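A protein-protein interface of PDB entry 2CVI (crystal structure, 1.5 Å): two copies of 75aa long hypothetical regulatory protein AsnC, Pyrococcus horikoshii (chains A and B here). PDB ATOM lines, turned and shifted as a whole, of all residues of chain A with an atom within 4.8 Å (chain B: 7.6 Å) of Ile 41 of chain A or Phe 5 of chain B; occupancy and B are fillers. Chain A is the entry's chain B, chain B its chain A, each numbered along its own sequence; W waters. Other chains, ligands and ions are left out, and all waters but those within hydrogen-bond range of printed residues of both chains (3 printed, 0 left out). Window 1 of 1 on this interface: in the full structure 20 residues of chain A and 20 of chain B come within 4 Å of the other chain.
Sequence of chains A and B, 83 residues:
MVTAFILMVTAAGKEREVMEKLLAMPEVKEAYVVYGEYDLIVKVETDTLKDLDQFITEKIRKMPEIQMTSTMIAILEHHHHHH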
ATOM      1  N   PHE A   5     -18.549  23.469   3.714  1.00  0.00           N
ATOM      2  CA  PHE A   5     -19.208  24.487   2.944  1.00  0.00           C
ATOM      3  C   PHE A   5     -18.089  25.361   2.439  1.00  0.00           C
ATOM      4  O   PHE A   5     -17.368  25.998   3.238  1.00  0.00           O
ATOM      5  CB  PHE A   5     -20.168  25.301   3.796  1.00  0.00           C
ATOM      6  CG  PHE A   5     -21.482  24.626   4.035  1.00  0.00           C
ATOM      7  CD1 PHE A   5     -22.539  24.818   3.122  1.00  0.00           C
ATOM      8  CD2 PHE A   5     -21.688  23.828   5.144  1.00  0.00           C
ATOM      9  CE1 PHE A   5     -23.765  24.233   3.320  1.00  0.00           C
ATOM     10  CE2 PHE A   5     -22.954  23.228   5.341  1.00  0.00           C
ATOM     11  CZ  PHE A   5     -23.968  23.458   4.406  1.00  0.00           C
ATOM     12  N   ILE A   6     -17.919  25.408   1.128  1.00  0.00           N
ATOM     13  CA  ILE A   6     -16.845  26.180   0.561  1.00  0.00           C
ATOM     14  C   ILE A   6     -17.385  27.393  -0.196  1.00  0.00           C
ATOM     15  O   ILE A   6     -18.138  27.247  -1.178  1.00  0.00           O
ATOM     16  CB  ILE A   6     -16.026  25.312  -0.418  1.00  0.00           C
ATOM     17  CG1 ILE A   6     -15.651  23.986   0.242  1.00  0.00           C
ATOM     18  CG2 ILE A   6     -14.798  26.047  -0.866  1.00  0.00           C
ATOM     19  CD1 ILE A   6     -14.823  23.092  -0.667  1.00  0.00           C
ATOM     20  N   LEU A   7     -16.990  28.586   0.245  1.00  0.00           N
ATOM     21  CA  LEU A   7     -17.379  29.835  -0.398  1.00  0.00           C
ATOM     22  C   LEU A   7     -16.332  30.005  -1.484  1.00  0.00           C
ATOM     23  O   LEU A   7     -15.163  29.724  -1.241  1.00  0.00           O
ATOM     24  CB  LEU A   7     -17.266  30.980   0.602  1.00  0.00           C
ATOM     25  CG  LEU A   7     -18.350  31.110   1.668  1.00  0.00           C
ATOM     26  CD1 LEU A   7     -18.684  29.777   2.290  1.00  0.00           C
ATOM     27  CD2 LEU A   7     -17.861  32.108   2.748  1.00  0.00           C
ATOM     28  N   GLU A  30     -24.689  19.892  -2.898  1.00  0.00           N
ATOM     29  CA  GLU A  30     -25.489  21.090  -3.224  1.00  0.00           C
ATOM     30  C   GLU A  30     -24.540  22.168  -3.679  1.00  0.00           C
ATOM     31  O   GLU A  30     -23.367  22.129  -3.339  1.00  0.00           O
ATOM     32  CB  GLU A  30     -26.257  21.625  -2.004  1.00  0.00           C
ATOM     33  CG  GLU A  30     -27.146  20.593  -1.354  1.00  0.00           C
ATOM     34  CD  GLU A  30     -27.808  21.093  -0.081  1.00  0.00           C
ATOM     35  OE1 GLU A  30     -28.448  20.264   0.609  1.00  0.00           O
ATOM     36  OE2 GLU A  30     -27.675  22.294   0.253  1.00  0.00           O
ATOM     37  N   ALA A  31     -25.022  23.116  -4.471  1.00  0.00           N
ATOM     38  CA  ALA A  31     -24.142  24.214  -4.900  1.00  0.00           C
ATOM     39  C   ALA A  31     -25.031  25.370  -5.293  1.00  0.00           C
ATOM     40  O   ALA A  31     -26.119  25.153  -5.826  1.00  0.00           O
ATOM     41  CB  ALA A  31     -23.227  23.792  -6.053  1.00  0.00           C
ATOM     42  N   TYR A  32     -24.590  26.587  -4.960  1.00  0.00           N
ATOM     43  CA  TYR A  32     -25.386  27.783  -5.182  1.00  0.00           C
ATOM     44  C   TYR A  32     -24.539  28.909  -5.709  1.00  0.00           C
ATOM     45  O   TYR A  32     -23.476  29.167  -5.148  1.00  0.00           O
ATOM     46  CB  TYR A  32     -25.956  28.294  -3.836  1.00  0.00           C
ATOM     47  CG  TYR A  32     -26.714  27.262  -3.029  1.00  0.00           C
ATOM     48  CD1 TYR A  32     -28.108  27.274  -2.982  1.00  0.00           C
ATOM     49  CD2 TYR A  32     -26.035  26.270  -2.306  1.00  0.00           C
ATOM     50  CE1 TYR A  32     -28.838  26.301  -2.246  1.00  0.00           C
ATOM     51  CE2 TYR A  32     -26.772  25.289  -1.554  1.00  0.00           C
ATOM     52  CZ  TYR A  32     -28.147  25.326  -1.549  1.00  0.00           C
ATOM     53  OH  TYR A  32     -28.906  24.396  -0.848  1.00  0.00           O
ATOM     54  N   VAL A  34     -24.303  32.713  -5.773  1.00  0.00           N
ATOM     55  CA  VAL A  34     -24.899  33.646  -4.825  1.00  0.00           C
ATOM     56  C   VAL A  34     -24.503  35.067  -5.113  1.00  0.00           C
ATOM     57  O   VAL A  34     -23.553  35.304  -5.847  1.00  0.00           O
ATOM     58  CB  VAL A  34     -24.466  33.307  -3.350  1.00  0.00           C
ATOM     59  CG1 VAL A  34     -24.953  31.927  -2.965  1.00  0.00           C
ATOM     60  CG2 VAL A  34     -22.932  33.309  -3.215  1.00  0.00           C
ATOM     61  N   ASP A  39     -18.991  34.301  -4.779  1.00  0.00           N
ATOM     62  CA  ASP A  39     -19.764  33.951  -5.971  1.00  0.00           C
ATOM     63  C   ASP A  39     -20.543  32.644  -5.845  1.00  0.00           C
ATOM     64  O   ASP A  39     -21.574  32.493  -6.489  1.00  0.00           O
ATOM     65  CB  ASP A  39     -18.863  33.831  -7.212  1.00  0.00           C
ATOM     66  CG  ASP A  39     -18.173  35.122  -7.568  1.00  0.00           C
ATOM     67  OD1 ASP A  39     -18.800  36.199  -7.458  1.00  0.00           O
ATOM     68  OD2 ASP A  39     -17.015  35.044  -8.015  1.00  0.00           O
ATOM     69  N   LEU A  40     -20.018  31.698  -5.069  1.00  0.00           N
ATOM     70  CA  LEU A  40     -20.719  30.421  -4.863  1.00  0.00           C
ATOM     71  C   LEU A  40     -20.526  29.950  -3.447  1.00  0.00           C
ATOM     72  O   LEU A  40     -19.582  30.323  -2.772  1.00  0.00           O
ATOM     73  CB  LEU A  40     -20.159  29.267  -5.724  1.00  0.00           C
ATOM     74  CG  LEU A  40     -20.542  29.204  -7.184  1.00  0.00           C
ATOM     75  CD1 LEU A  40     -19.535  29.977  -8.000  1.00  0.00           C
ATOM     76  CD2 LEU A  40     -20.611  27.723  -7.605  1.00  0.00           C
ATOM     77  N   ILE A  41     -21.438  29.100  -3.020  1.00  0.00           N
ATOM     78  CA  ILE A  41     -21.295  28.377  -1.763  1.00  0.00           C
ATOM     79  C   ILE A  41     -21.589  26.937  -2.183  1.00  0.00           C
ATOM     80  O   ILE A  41     -22.594  26.653  -2.862  1.00  0.00           O
ATOM     81  CB  ILE A  41     -22.194  28.879  -0.609  1.00  0.00           C
ATOM     82  CG1 ILE A  41     -21.879  28.046   0.645  1.00  0.00           C
ATOM     83  CG2 ILE A  41     -23.649  28.737  -0.912  1.00  0.00           C
ATOM     84  CD1 ILE A  41     -22.421  28.625   1.976  1.00  0.00           C
ATOM     85  N   VAL A  42     -20.666  26.037  -1.824  1.00  0.00           N
ATOM     86  CA  VAL A  42     -20.764  24.642  -2.265  1.00  0.00           C
ATOM     87  C   VAL A  42     -20.735  23.707  -1.090  1.00  0.00           C
ATOM     88  O   VAL A  42     -19.913  23.896  -0.172  1.00  0.00           O
ATOM     89  CB  VAL A  42     -19.575  24.346  -3.160  1.00  0.00           C
ATOM     90  CG1 VAL A  42     -19.662  22.883  -3.672  1.00  0.00           C
ATOM     91  CG2 VAL A  42     -19.535  25.360  -4.342  1.00  0.00           C
ATOM     92  N   LYS A  43     -21.607  22.701  -1.065  1.00  0.00           N
ATOM     93  CA  LYS A  43     -21.684  21.773   0.066  1.00  0.00           C
ATOM     94  C   LYS A  43     -21.103  20.427  -0.348  1.00  0.00           C
ATOM     95  O   LYS A  43     -21.592  19.809  -1.295  1.00  0.00           O
ATOM     96  CB  LYS A  43     -23.125  21.571   0.514  1.00  0.00           C
ATOM     97  CG  LYS A  43     -23.231  20.739   1.816  1.00  0.00           C
ATOM     98  CD  LYS A  43     -24.683  20.394   2.184  1.00  0.00           C
ATOM     99  CE  LYS A  43     -24.800  19.814   3.573  1.00  0.00           C
ATOM    100  NZ  LYS A  43     -26.184  19.316   3.898  1.00  0.00           N
ATOM    101  N   THR B   3     -33.930  32.250  -1.036  1.00  0.00           N
ATOM    102  CA  THR B   3     -33.112  31.280  -0.335  1.00  0.00           C
ATOM    103  C   THR B   3     -31.761  31.945  -0.081  1.00  0.00           C
ATOM    104  O   THR B   3     -31.186  32.547  -0.979  1.00  0.00           O
ATOM    105  CB  THR B   3     -32.896  30.037  -1.206  1.00  0.00           C
ATOM    106  OG1 THR B   3     -34.178  29.436  -1.436  1.00  0.00           O
ATOM    107  CG2 THR B   3     -31.990  29.034  -0.513  1.00  0.00           C
ATOM    108  N   ALA B   4     -31.266  31.828   1.143  1.00  0.00           N
ATOM    109  CA  ALA B   4     -29.981  32.454   1.455  1.00  0.00           C
ATOM    110  C   ALA B   4     -29.228  31.694   2.527  1.00  0.00           C
ATOM    111  O   ALA B   4     -29.811  30.940   3.288  1.00  0.00           O
ATOM    112  CB  ALA B   4     -30.215  33.924   1.931  1.00  0.00           C
ATOM    113  N   PHE B   5     -27.913  31.864   2.547  1.00  0.00           N
ATOM    114  CA  PHE B   5     -27.090  31.281   3.592  1.00  0.00           C
ATOM    115  C   PHE B   5     -26.528  32.446   4.386  1.00  0.00           C
ATOM    116  O   PHE B   5     -25.972  33.385   3.803  1.00  0.00           O
ATOM    117  CB  PHE B   5     -25.927  30.489   2.999  1.00  0.00           C
ATOM    118  CG  PHE B   5     -26.325  29.150   2.500  1.00  0.00           C
ATOM    119  CD1 PHE B   5     -26.270  28.038   3.344  1.00  0.00           C
ATOM    120  CD2 PHE B   5     -26.821  29.007   1.212  1.00  0.00           C
ATOM    121  CE1 PHE B   5     -26.713  26.812   2.931  1.00  0.00           C
ATOM    122  CE2 PHE B   5     -27.277  27.779   0.748  1.00  0.00           C
ATOM    123  CZ  PHE B   5     -27.231  26.660   1.614  1.00  0.00           C
ATOM    124  N   ILE B   6     -26.716  32.407   5.698  1.00  0.00           N
ATOM    125  CA  ILE B   6     -26.189  33.473   6.553  1.00  0.00           C
ATOM    126  C   ILE B   6     -24.975  32.890   7.296  1.00  0.00           C
ATOM    127  O   ILE B   6     -25.132  31.893   8.025  1.00  0.00           O
ATOM    128  CB  ILE B   6     -27.231  33.945   7.585  1.00  0.00           C
ATOM    129  CG1 ILE B   6     -28.532  34.424   6.921  1.00  0.00           C
ATOM    130  CG2 ILE B   6     -26.608  35.150   8.375  1.00  0.00           C
ATOM    131  CD1 ILE B   6     -29.644  34.719   7.937  1.00  0.00           C
ATOM    132  N   LEU B   7     -23.793  33.468   7.099  1.00  0.00           N
ATOM    133  CA  LEU B   7     -22.559  33.009   7.748  1.00  0.00           C
ATOM    134  C   LEU B   7     -22.391  33.877   8.977  1.00  0.00           C
ATOM    135  O   LEU B   7     -22.461  35.101   8.874  1.00  0.00           O
ATOM    136  CB  LEU B   7     -21.356  33.153   6.794  1.00  0.00           C
ATOM    137  CG  LEU B   7     -21.182  32.268   5.541  1.00  0.00           C
ATOM    138  CD1 LEU B   7     -20.846  30.857   5.934  1.00  0.00           C
ATOM    139  CD2 LEU B   7     -22.388  32.351   4.620  1.00  0.00           C
ATOM    140  N   MET B   8     -22.166  33.256  10.131  1.00  0.00           N
ATOM    141  CA  MET B   8     -22.112  33.981  11.389  1.00  0.00           C
ATOM    142  C   MET B   8     -20.869  33.803  12.219  1.00  0.00           C
ATOM    143  O   MET B   8     -20.290  32.712  12.267  1.00  0.00           O
ATOM    144  CB  MET B   8     -23.293  33.567  12.269  1.00  0.00           C
ATOM    145  CG  MET B   8     -24.672  33.582  11.540  1.00  0.00           C
ATOM    146  SD  MET B   8     -25.954  33.153  12.735  1.00  0.00           S
ATOM    147  CE  MET B   8     -27.463  33.378  11.684  1.00  0.00           C
ATOM    148  N   GLU B  30     -31.955  25.023   8.020  1.00  0.00           N
ATOM    149  CA  GLU B  30     -30.822  24.173   8.369  1.00  0.00           C
ATOM    150  C   GLU B  30     -29.824  25.061   9.081  1.00  0.00           C
ATOM    151  O   GLU B  30     -29.763  26.258   8.814  1.00  0.00           O
ATOM    152  CB  GLU B  30     -30.087  23.641   7.128  1.00  0.00           C
ATOM    153  CG  GLU B  30     -30.964  22.909   6.168  1.00  0.00           C
ATOM    154  CD  GLU B  30     -30.251  22.575   4.881  1.00  0.00           C
ATOM    155  OE1 GLU B  30     -29.004  22.650   4.831  1.00  0.00           O
ATOM    156  OE2 GLU B  30     -30.953  22.221   3.914  1.00  0.00           O
ATOM    157  N   TYR B  32     -25.643  24.748  10.900  1.00  0.00           N
ATOM    158  CA  TYR B  32     -24.456  23.952  11.145  1.00  0.00           C
ATOM    159  C   TYR B  32     -23.428  24.723  11.923  1.00  0.00           C
ATOM    160  O   TYR B  32     -23.098  25.853  11.575  1.00  0.00           O
ATOM    161  CB  TYR B  32     -23.776  23.575   9.839  1.00  0.00           C
ATOM    162  CG  TYR B  32     -24.665  22.880   8.857  1.00  0.00           C
ATOM    163  CD1 TYR B  32     -24.616  21.503   8.700  1.00  0.00           C
ATOM    164  CD2 TYR B  32     -25.523  23.618   8.049  1.00  0.00           C
ATOM    165  CE1 TYR B  32     -25.432  20.872   7.719  1.00  0.00           C
ATOM    166  CE2 TYR B  32     -26.321  23.011   7.089  1.00  0.00           C
ATOM    167  CZ  TYR B  32     -26.268  21.648   6.937  1.00  0.00           C
ATOM    168  OH  TYR B  32     -27.104  21.108   5.978  1.00  0.00           O
ATOM    169  N   LEU B  40     -20.894  29.609  12.422  1.00  0.00           N
ATOM    170  CA  LEU B  40     -22.190  28.995  12.183  1.00  0.00           C
ATOM    171  C   LEU B  40     -22.664  29.344  10.791  1.00  0.00           C
ATOM    172  O   LEU B  40     -22.425  30.444  10.311  1.00  0.00           O
ATOM    173  CB  LEU B  40     -23.219  29.514  13.226  1.00  0.00           C
ATOM    174  CG  LEU B  40     -24.649  28.963  13.354  1.00  0.00           C
ATOM    175  CD1 LEU B  40     -24.612  27.452  13.571  1.00  0.00           C
ATOM    176  CD2 LEU B  40     -25.358  29.661  14.529  1.00  0.00           C
ATOM    177  N   ILE B  41     -23.297  28.384  10.118  1.00  0.00           N
ATOM    178  CA  ILE B  41     -23.871  28.631   8.795  1.00  0.00           C
ATOM    179  C   ILE B  41     -25.336  28.228   8.886  1.00  0.00           C
ATOM    180  O   ILE B  41     -25.665  27.138   9.334  1.00  0.00           O
ATOM    181  CB  ILE B  41     -23.253  27.790   7.709  1.00  0.00           C
ATOM    182  CG1 ILE B  41     -21.809  28.181   7.510  1.00  0.00           C
ATOM    183  CG2 ILE B  41     -24.052  28.028   6.359  1.00  0.00           C
ATOM    184  CD1 ILE B  41     -21.142  27.384   6.433  1.00  0.00           C
ATOM    185  N   VAL B  42     -26.213  29.114   8.442  1.00  0.00           N
ATOM    186  CA  VAL B  42     -27.639  28.846   8.510  1.00  0.00           C
ATOM    187  C   VAL B  42     -28.271  29.061   7.137  1.00  0.00           C
ATOM    188  O   VAL B  42     -27.910  30.000   6.410  1.00  0.00           O
ATOM    189  CB  VAL B  42     -28.287  29.763   9.567  1.00  0.00           C
ATOM    190  CG1 VAL B  42     -27.405  29.747  10.846  1.00  0.00           C
ATOM    191  CG2 VAL B  42     -28.469  31.170   9.052  1.00  0.00           C
ATOM    192  N   LYS B  43     -29.152  28.148   6.733  1.00  0.00           N
ATOM    193  CA  LYS B  43     -29.849  28.269   5.448  1.00  0.00           C
ATOM    194  C   LYS B  43     -31.237  28.771   5.810  1.00  0.00           C
ATOM    195  O   LYS B  43     -31.937  28.167   6.625  1.00  0.00           O
ATOM    196  CB  LYS B  43     -29.988  26.920   4.680  1.00  0.00           C
ATOM    197  CG  LYS B  43     -30.527  27.108   3.232  1.00  0.00           C
ATOM    198  CD  LYS B  43     -30.766  25.774   2.475  1.00  0.00           C
ATOM    199  CE  LYS B  43     -31.113  26.015   1.011  1.00  0.00           C
ATOM    200  NZ  LYS B  43     -31.655  24.743   0.422  1.00  0.00           N
ATOM    201  N   VAL B  44     -31.629  29.888   5.206  1.00  0.00           N
ATOM    202  CA  VAL B  44     -32.958  30.453   5.432  1.00  0.00           C
ATOM    203  C   VAL B  44     -33.722  30.607   4.123  1.00  0.00           C
ATOM    204  O   VAL B  44     -33.148  30.709   3.034  1.00  0.00           O
ATOM    205  CB  VAL B  44     -32.891  31.855   6.062  1.00  0.00           C
ATOM    206  CG1 VAL B  44     -32.276  31.795   7.430  1.00  0.00           C
ATOM    207  CG2 VAL B  44     -32.096  32.776   5.185  1.00  0.00           C
ATOM    208  N   GLU B  45     -35.044  30.537   4.251  1.00  0.00           N
ATOM    209  CA  GLU B  45     -35.960  30.778   3.137  1.00  0.00           C
ATOM    210  C   GLU B  45     -36.998  31.791   3.657  1.00  0.00           C
ATOM    211  O   GLU B  45     -37.556  31.636   4.752  1.00  0.00           O
ATOM    212  CB  GLU B  45     -36.640  29.460   2.673  1.00  0.00           C
ATOM    213  CG  GLU B  45     -35.659  28.468   2.059  1.00  0.00           C
ATOM    214  CD  GLU B  45     -36.271  27.097   1.741  1.00  0.00           C
ATOM    215  OE1 GLU B  45     -37.324  26.765   2.315  1.00  0.00           O
ATOM    216  OE2 GLU B  45     -35.679  26.365   0.928  1.00  0.00           O
ATOM    217  N   LEU B  52     -36.113  38.848   4.335  1.00  0.00           N
ATOM    218  CA  LEU B  52     -34.764  38.397   4.680  1.00  0.00           C
ATOM    219  C   LEU B  52     -33.980  39.528   5.355  1.00  0.00           C
ATOM    220  O   LEU B  52     -33.256  39.277   6.315  1.00  0.00           O
ATOM    221  CB  LEU B  52     -34.057  37.910   3.420  1.00  0.00           C
ATOM    222  CG  LEU B  52     -32.573  37.564   3.605  1.00  0.00           C
ATOM    223  CD1 LEU B  52     -32.435  36.427   4.635  1.00  0.00           C
ATOM    224  CD2 LEU B  52     -31.949  37.225   2.235  1.00  0.00           C
ATOM    225  N   ILE B  56     -32.253  39.453   9.111  1.00  0.00           N
ATOM    226  CA  ILE B  56     -30.842  39.712   9.351  1.00  0.00           C
ATOM    227  C   ILE B  56     -30.583  40.900  10.265  1.00  0.00           C
ATOM    228  O   ILE B  56     -29.736  40.813  11.146  1.00  0.00           O
ATOM    229  CB  ILE B  56     -30.127  39.976   7.991  1.00  0.00           C
ATOM    230  CG1 ILE B  56     -30.062  38.671   7.189  1.00  0.00           C
ATOM    231  CG2 ILE B  56     -28.720  40.569   8.212  1.00  0.00           C
ATOM    232  CD1 ILE B  56     -29.540  38.846   5.782  1.00  0.00           C
ATOM    233  N   SER B  70     -22.692  37.655   7.465  1.00  0.00           N
ATOM    234  CA  SER B  70     -22.478  37.952   6.036  1.00  0.00           C
ATOM    235  C   SER B  70     -23.458  37.015   5.328  1.00  0.00           C
ATOM    236  O   SER B  70     -23.359  35.790   5.478  1.00  0.00           O
ATOM    237  CB  SER B  70     -21.051  37.664   5.571  1.00  0.00           C
ATOM    238  OG  SER B  70     -20.882  38.036   4.206  1.00  0.00           O
ATOM    239  N   THR B  71     -24.367  37.566   4.539  1.00  0.00           N
ATOM    240  CA  THR B  71     -25.400  36.742   3.892  1.00  0.00           C
ATOM    241  C   THR B  71     -25.188  36.585   2.387  1.00  0.00           C
ATOM    242  O   THR B  71     -24.864  37.559   1.690  1.00  0.00           O
ATOM    243  CB  THR B  71     -26.754  37.351   4.179  1.00  0.00           C
ATOM    244  OG1 THR B  71     -26.955  37.402   5.599  1.00  0.00           O
ATOM    245  CG2 THR B  71     -27.901  36.519   3.559  1.00  0.00           C
ATOM    246  N   MET B  72     -25.338  35.353   1.902  1.00  0.00           N
ATOM    247  CA  MET B  72     -25.154  35.033   0.464  1.00  0.00           C
ATOM    248  C   MET B  72     -26.549  34.693  -0.093  1.00  0.00           C
ATOM    249  O   MET B  72     -27.117  33.690   0.329  1.00  0.00           O
ATOM    250  CB  MET B  72     -24.264  33.790   0.316  1.00  0.00           C
ATOM    251  CG  MET B  72     -22.934  33.794   1.079  1.00  0.00           C
ATOM    252  SD  MET B  72     -21.761  34.968   0.411  1.00  0.00           S
ATOM    253  CE  MET B  72     -20.785  35.269   1.940  1.00  0.00           C
ATOM    254  N   ILE B  73     -27.125  35.526  -0.984  1.00  0.00           N
ATOM    255  CA  ILE B  73     -28.466  35.243  -1.573  1.00  0.00           C
ATOM    256  C   ILE B  73     -28.328  34.307  -2.768  1.00  0.00           C
ATOM    257  O   ILE B  73     -27.591  34.594  -3.704  1.00  0.00           O
ATOM    258  CB  ILE B  73     -29.161  36.545  -2.064  1.00  0.00           C
ATOM    259  CG1 ILE B  73     -29.375  37.513  -0.905  1.00  0.00           C
ATOM    260  CG2 ILE B  73     -30.493  36.215  -2.708  1.00  0.00           C
ATOM    261  CD1 ILE B  73     -29.712  38.942  -1.348  1.00  0.00           C
ATOM    262  N   ALA B  74     -29.037  33.186  -2.749  1.00  0.00           N
ATOM    263  CA  ALA B  74     -28.949  32.253  -3.883  1.00  0.00           C
ATOM    264  C   ALA B  74     -29.652  32.838  -5.117  1.00  0.00           C
ATOM    265  O   ALA B  74     -30.815  33.265  -5.026  1.00  0.00           O
ATOM    266  CB  ALA B  74     -29.590  30.926  -3.482  1.00  0.00           C
ATOM    267  N   LEU B  76     -28.865  31.075  -8.223  1.00  0.00           N
ATOM    268  CA  LEU B  76     -28.916  29.888  -9.077  1.00  0.00           C
ATOM    269  C   LEU B  76     -28.459  28.741  -8.154  1.00  0.00           C
ATOM    270  O   LEU B  76     -27.602  28.914  -7.283  1.00  0.00           O
ATOM    271  CB  LEU B  76     -27.943  30.010 -10.258  1.00  0.00           C
ATOM    272  CG  LEU B  76     -28.264  29.010 -11.403  1.00  0.00           C
ATOM    273  CD1 LEU B  76     -29.472  29.486 -12.192  1.00  0.00           C
ATOM    274  CD2 LEU B  76     -27.062  28.842 -12.314  1.00  0.00           C
ATOM    275  N   GLU B  77     -29.017  27.546  -8.340  1.00  0.00           N
ATOM    276  CA  GLU B  77     -28.573  26.415  -7.530  1.00  0.00           C
ATOM    277  C   GLU B  77     -28.800  25.077  -8.206  1.00  0.00           C
ATOM    278  O   GLU B  77     -29.128  25.035  -9.394  1.00  0.00           O
ATOM    279  CB  GLU B  77     -29.129  26.472  -6.086  1.00  0.00           C
ATOM    280  CG  GLU B  77     -30.583  26.806  -5.916  1.00  0.00           C
ATOM    281  CD  GLU B  77     -31.446  25.641  -6.216  1.00  0.00           C
ATOM    282  OE1 GLU B  77     -31.866  24.965  -5.266  1.00  0.00           O
ATOM    283  OE2 GLU B  77     -31.674  25.408  -7.417  1.00  0.00           O
ATOM    284  N   HIS B  78     -28.661  23.996  -7.447  1.00  0.00           N
ATOM    285  CA  HIS B  78     -28.668  22.669  -8.039  1.00  0.00           C
ATOM    286  C   HIS B  78     -29.938  22.175  -8.650  1.00  0.00           C
ATOM    287  O   HIS B  78     -29.940  21.142  -9.310  1.00  0.00           O
ATOM    288  CB  HIS B  78     -28.071  21.660  -7.046  1.00  0.00           C
ATOM    289  CG  HIS B  78     -28.698  21.718  -5.708  1.00  0.00           C
ATOM    290  ND1 HIS B  78     -28.377  22.698  -4.800  1.00  0.00           N
ATOM    291  CD2 HIS B  78     -29.670  20.968  -5.132  1.00  0.00           C
ATOM    292  CE1 HIS B  78     -29.118  22.551  -3.717  1.00  0.00           C
ATOM    293  NE2 HIS B  78     -29.913  21.505  -3.896  1.00  0.00           N
HETATM  294  O   HOH W   1     -27.185  23.008   2.869  1.00  0.00           O
HETATM  295  O   HOH W   2     -28.827  19.923   3.202  1.00  0.00           O
HETATM  296  O   HOH W   3     -30.490  22.341   1.397  1.00  0.00           O
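Water W3 lies within hydrogen-bond range of the side-chain carboxylate of Glu 30 of chain B (2.6 Å), the side-chain amino group of Lys 43 of chain B (2.8 Å), the side-chain carboxylate of Glu 30 of chain A (3.0 Å) and the side-chain hydroxyl of Tyr 32 of chain A (3.4 Å). Water W2 lies within hydrogen-bond range of OE1 of Glu 30 of chain A, NZ of Lys 43 of chain A, OE1 of Glu 30 of chain B and OH of Tyr 32 of chain B. Water W1 lies within hydrogen-bond range of OE1 of Glu 30 of chain B and OE2 of Glu 30 of chain A.
Of the 24 printed residues of chain B, 10 touch a printed residue of chain A. Hydrophobic or aromatic side chains of chain B that line the printed part of chain A: Phe 5, Tyr 32, Ile 41, Met 72, Ala 74 and His 78.
The backbone NH (N) of Lys 43 of chain B sits at hydrogen-bond distance from the backbone carbonyl oxygen (O) of Glu 30 of chain B, 2.9 Å away. The backbone NH of Tyr 32 of chain B lies within hydrogen-bond range of the backbone carbonyl oxygen of Ile 41 of chain B (2.9 Å). The side-chain hydroxyl of Tyr 32 of chain A sits at hydrogen-bond distance from the side-chain carboxylate of Glu 30 of chain A (2.7 Å). O of Glu 30 of chain A sits at hydrogen-bond distance from N of Lys 43 of chain A, at 2.9 Å. N of Tyr 32 of chain A is in hydrogen-bond range of O of Ile 41 of chain A (2.9 Å).
The side-chain amino group (NZ) of Lys 43 of chain A lies within hydrogen-bond range of the side-chain hydroxyl (OH) of Tyr 32 of chain B, at 2.9 Å. NZ of Lys 43 of chain B is in hydrogen-bond range of OH of Tyr 32 of chain A. The backbone carbonyl oxygen (O) of Ala 31 of chain A is in hydrogen-bond range of the backbone NH (N) of His 78 of chain B.
Phe 5 of chain B touches its own counterpart, Phe 5 of chain A. Phe 5 of chain A touches Tyr 32 of chain B, and with the chains exchanged Tyr 32 of chain A touches Phe 5 of chain B. Phe 5 of chain A touches Ile 41 of chain B, and with the chains exchanged Ile 41 of chain A touches Phe 5 of chain B. Tyr 32 of chain A touches Lys 43 of chain B, and with the chains exchanged Lys 43 of chain A touches Tyr 32 of chain B. Positions printed for both chains: 5, 6, 7, 30, 32, 40, 41, 42 and 43.
Ile 41 of chain A touches just one residue of chain B: Phe 5. Of chain A, only Phe 5 (3.9 Å), Tyr 32 (3.4 Å) and Ile 41 (3.8 Å) come within 4 Å of Phe 5 of chain B. Of the printed residues of chain B, Ala 31 of chain A touches Glu 77 and His 78. Printed residues of chain B within 4 Å of Phe 5 of chain A: Phe 5, Tyr 32 and Ile 41. Of the printed residues of chain A, Glu 77 of chain B touches Ala 31 and Tyr 32. Of the printed residues of chain A, His 78 of chain B touches Glu 30 (3.5 Å), Ala 31 (3.2 Å) and Tyr 32 (3.4 Å). Of the printed residues of chain A, Leu 76 of chain B touches Tyr 32. Leu 7 of chain A touches none of the printed residues of chain B. Val 42 of chain A touches none of the printed residues of chain B. The nearest residue of chain B that does not touch Ile 41 of chain A is Leu 7 of chain B (4.6 Å). The nearest residue of chain A that does not touch Phe 5 of chain B is Glu 30 of chain A (4.6 Å).
Among the printed residues, pairs that only touch across the chains: Phe 5 of chain A with Phe 5 of chain B, Phe 5 of chain A with Tyr 32 of chain B, Phe 5 of chain A with Ile 41 of chain B, Glu 30 of chain A with His 78 of chain B, Ala 31 of chain A with Glu 77 of chain B, Tyr 32 of chain A with Phe 5 of chain B, Tyr 32 of chain A with Ala 74 of chain B, Tyr 32 of chain A with Leu 76 of chain B, Tyr 32 of chain A with Glu 77 of chain B, Tyr 32 of chain A with His 78 of chain B, Val 34 of chain A with Met 72 of chain B, Val 34 of chain A with Ile 73 of chain B and Ile 41 of chain A with Phe 5 of chain B.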
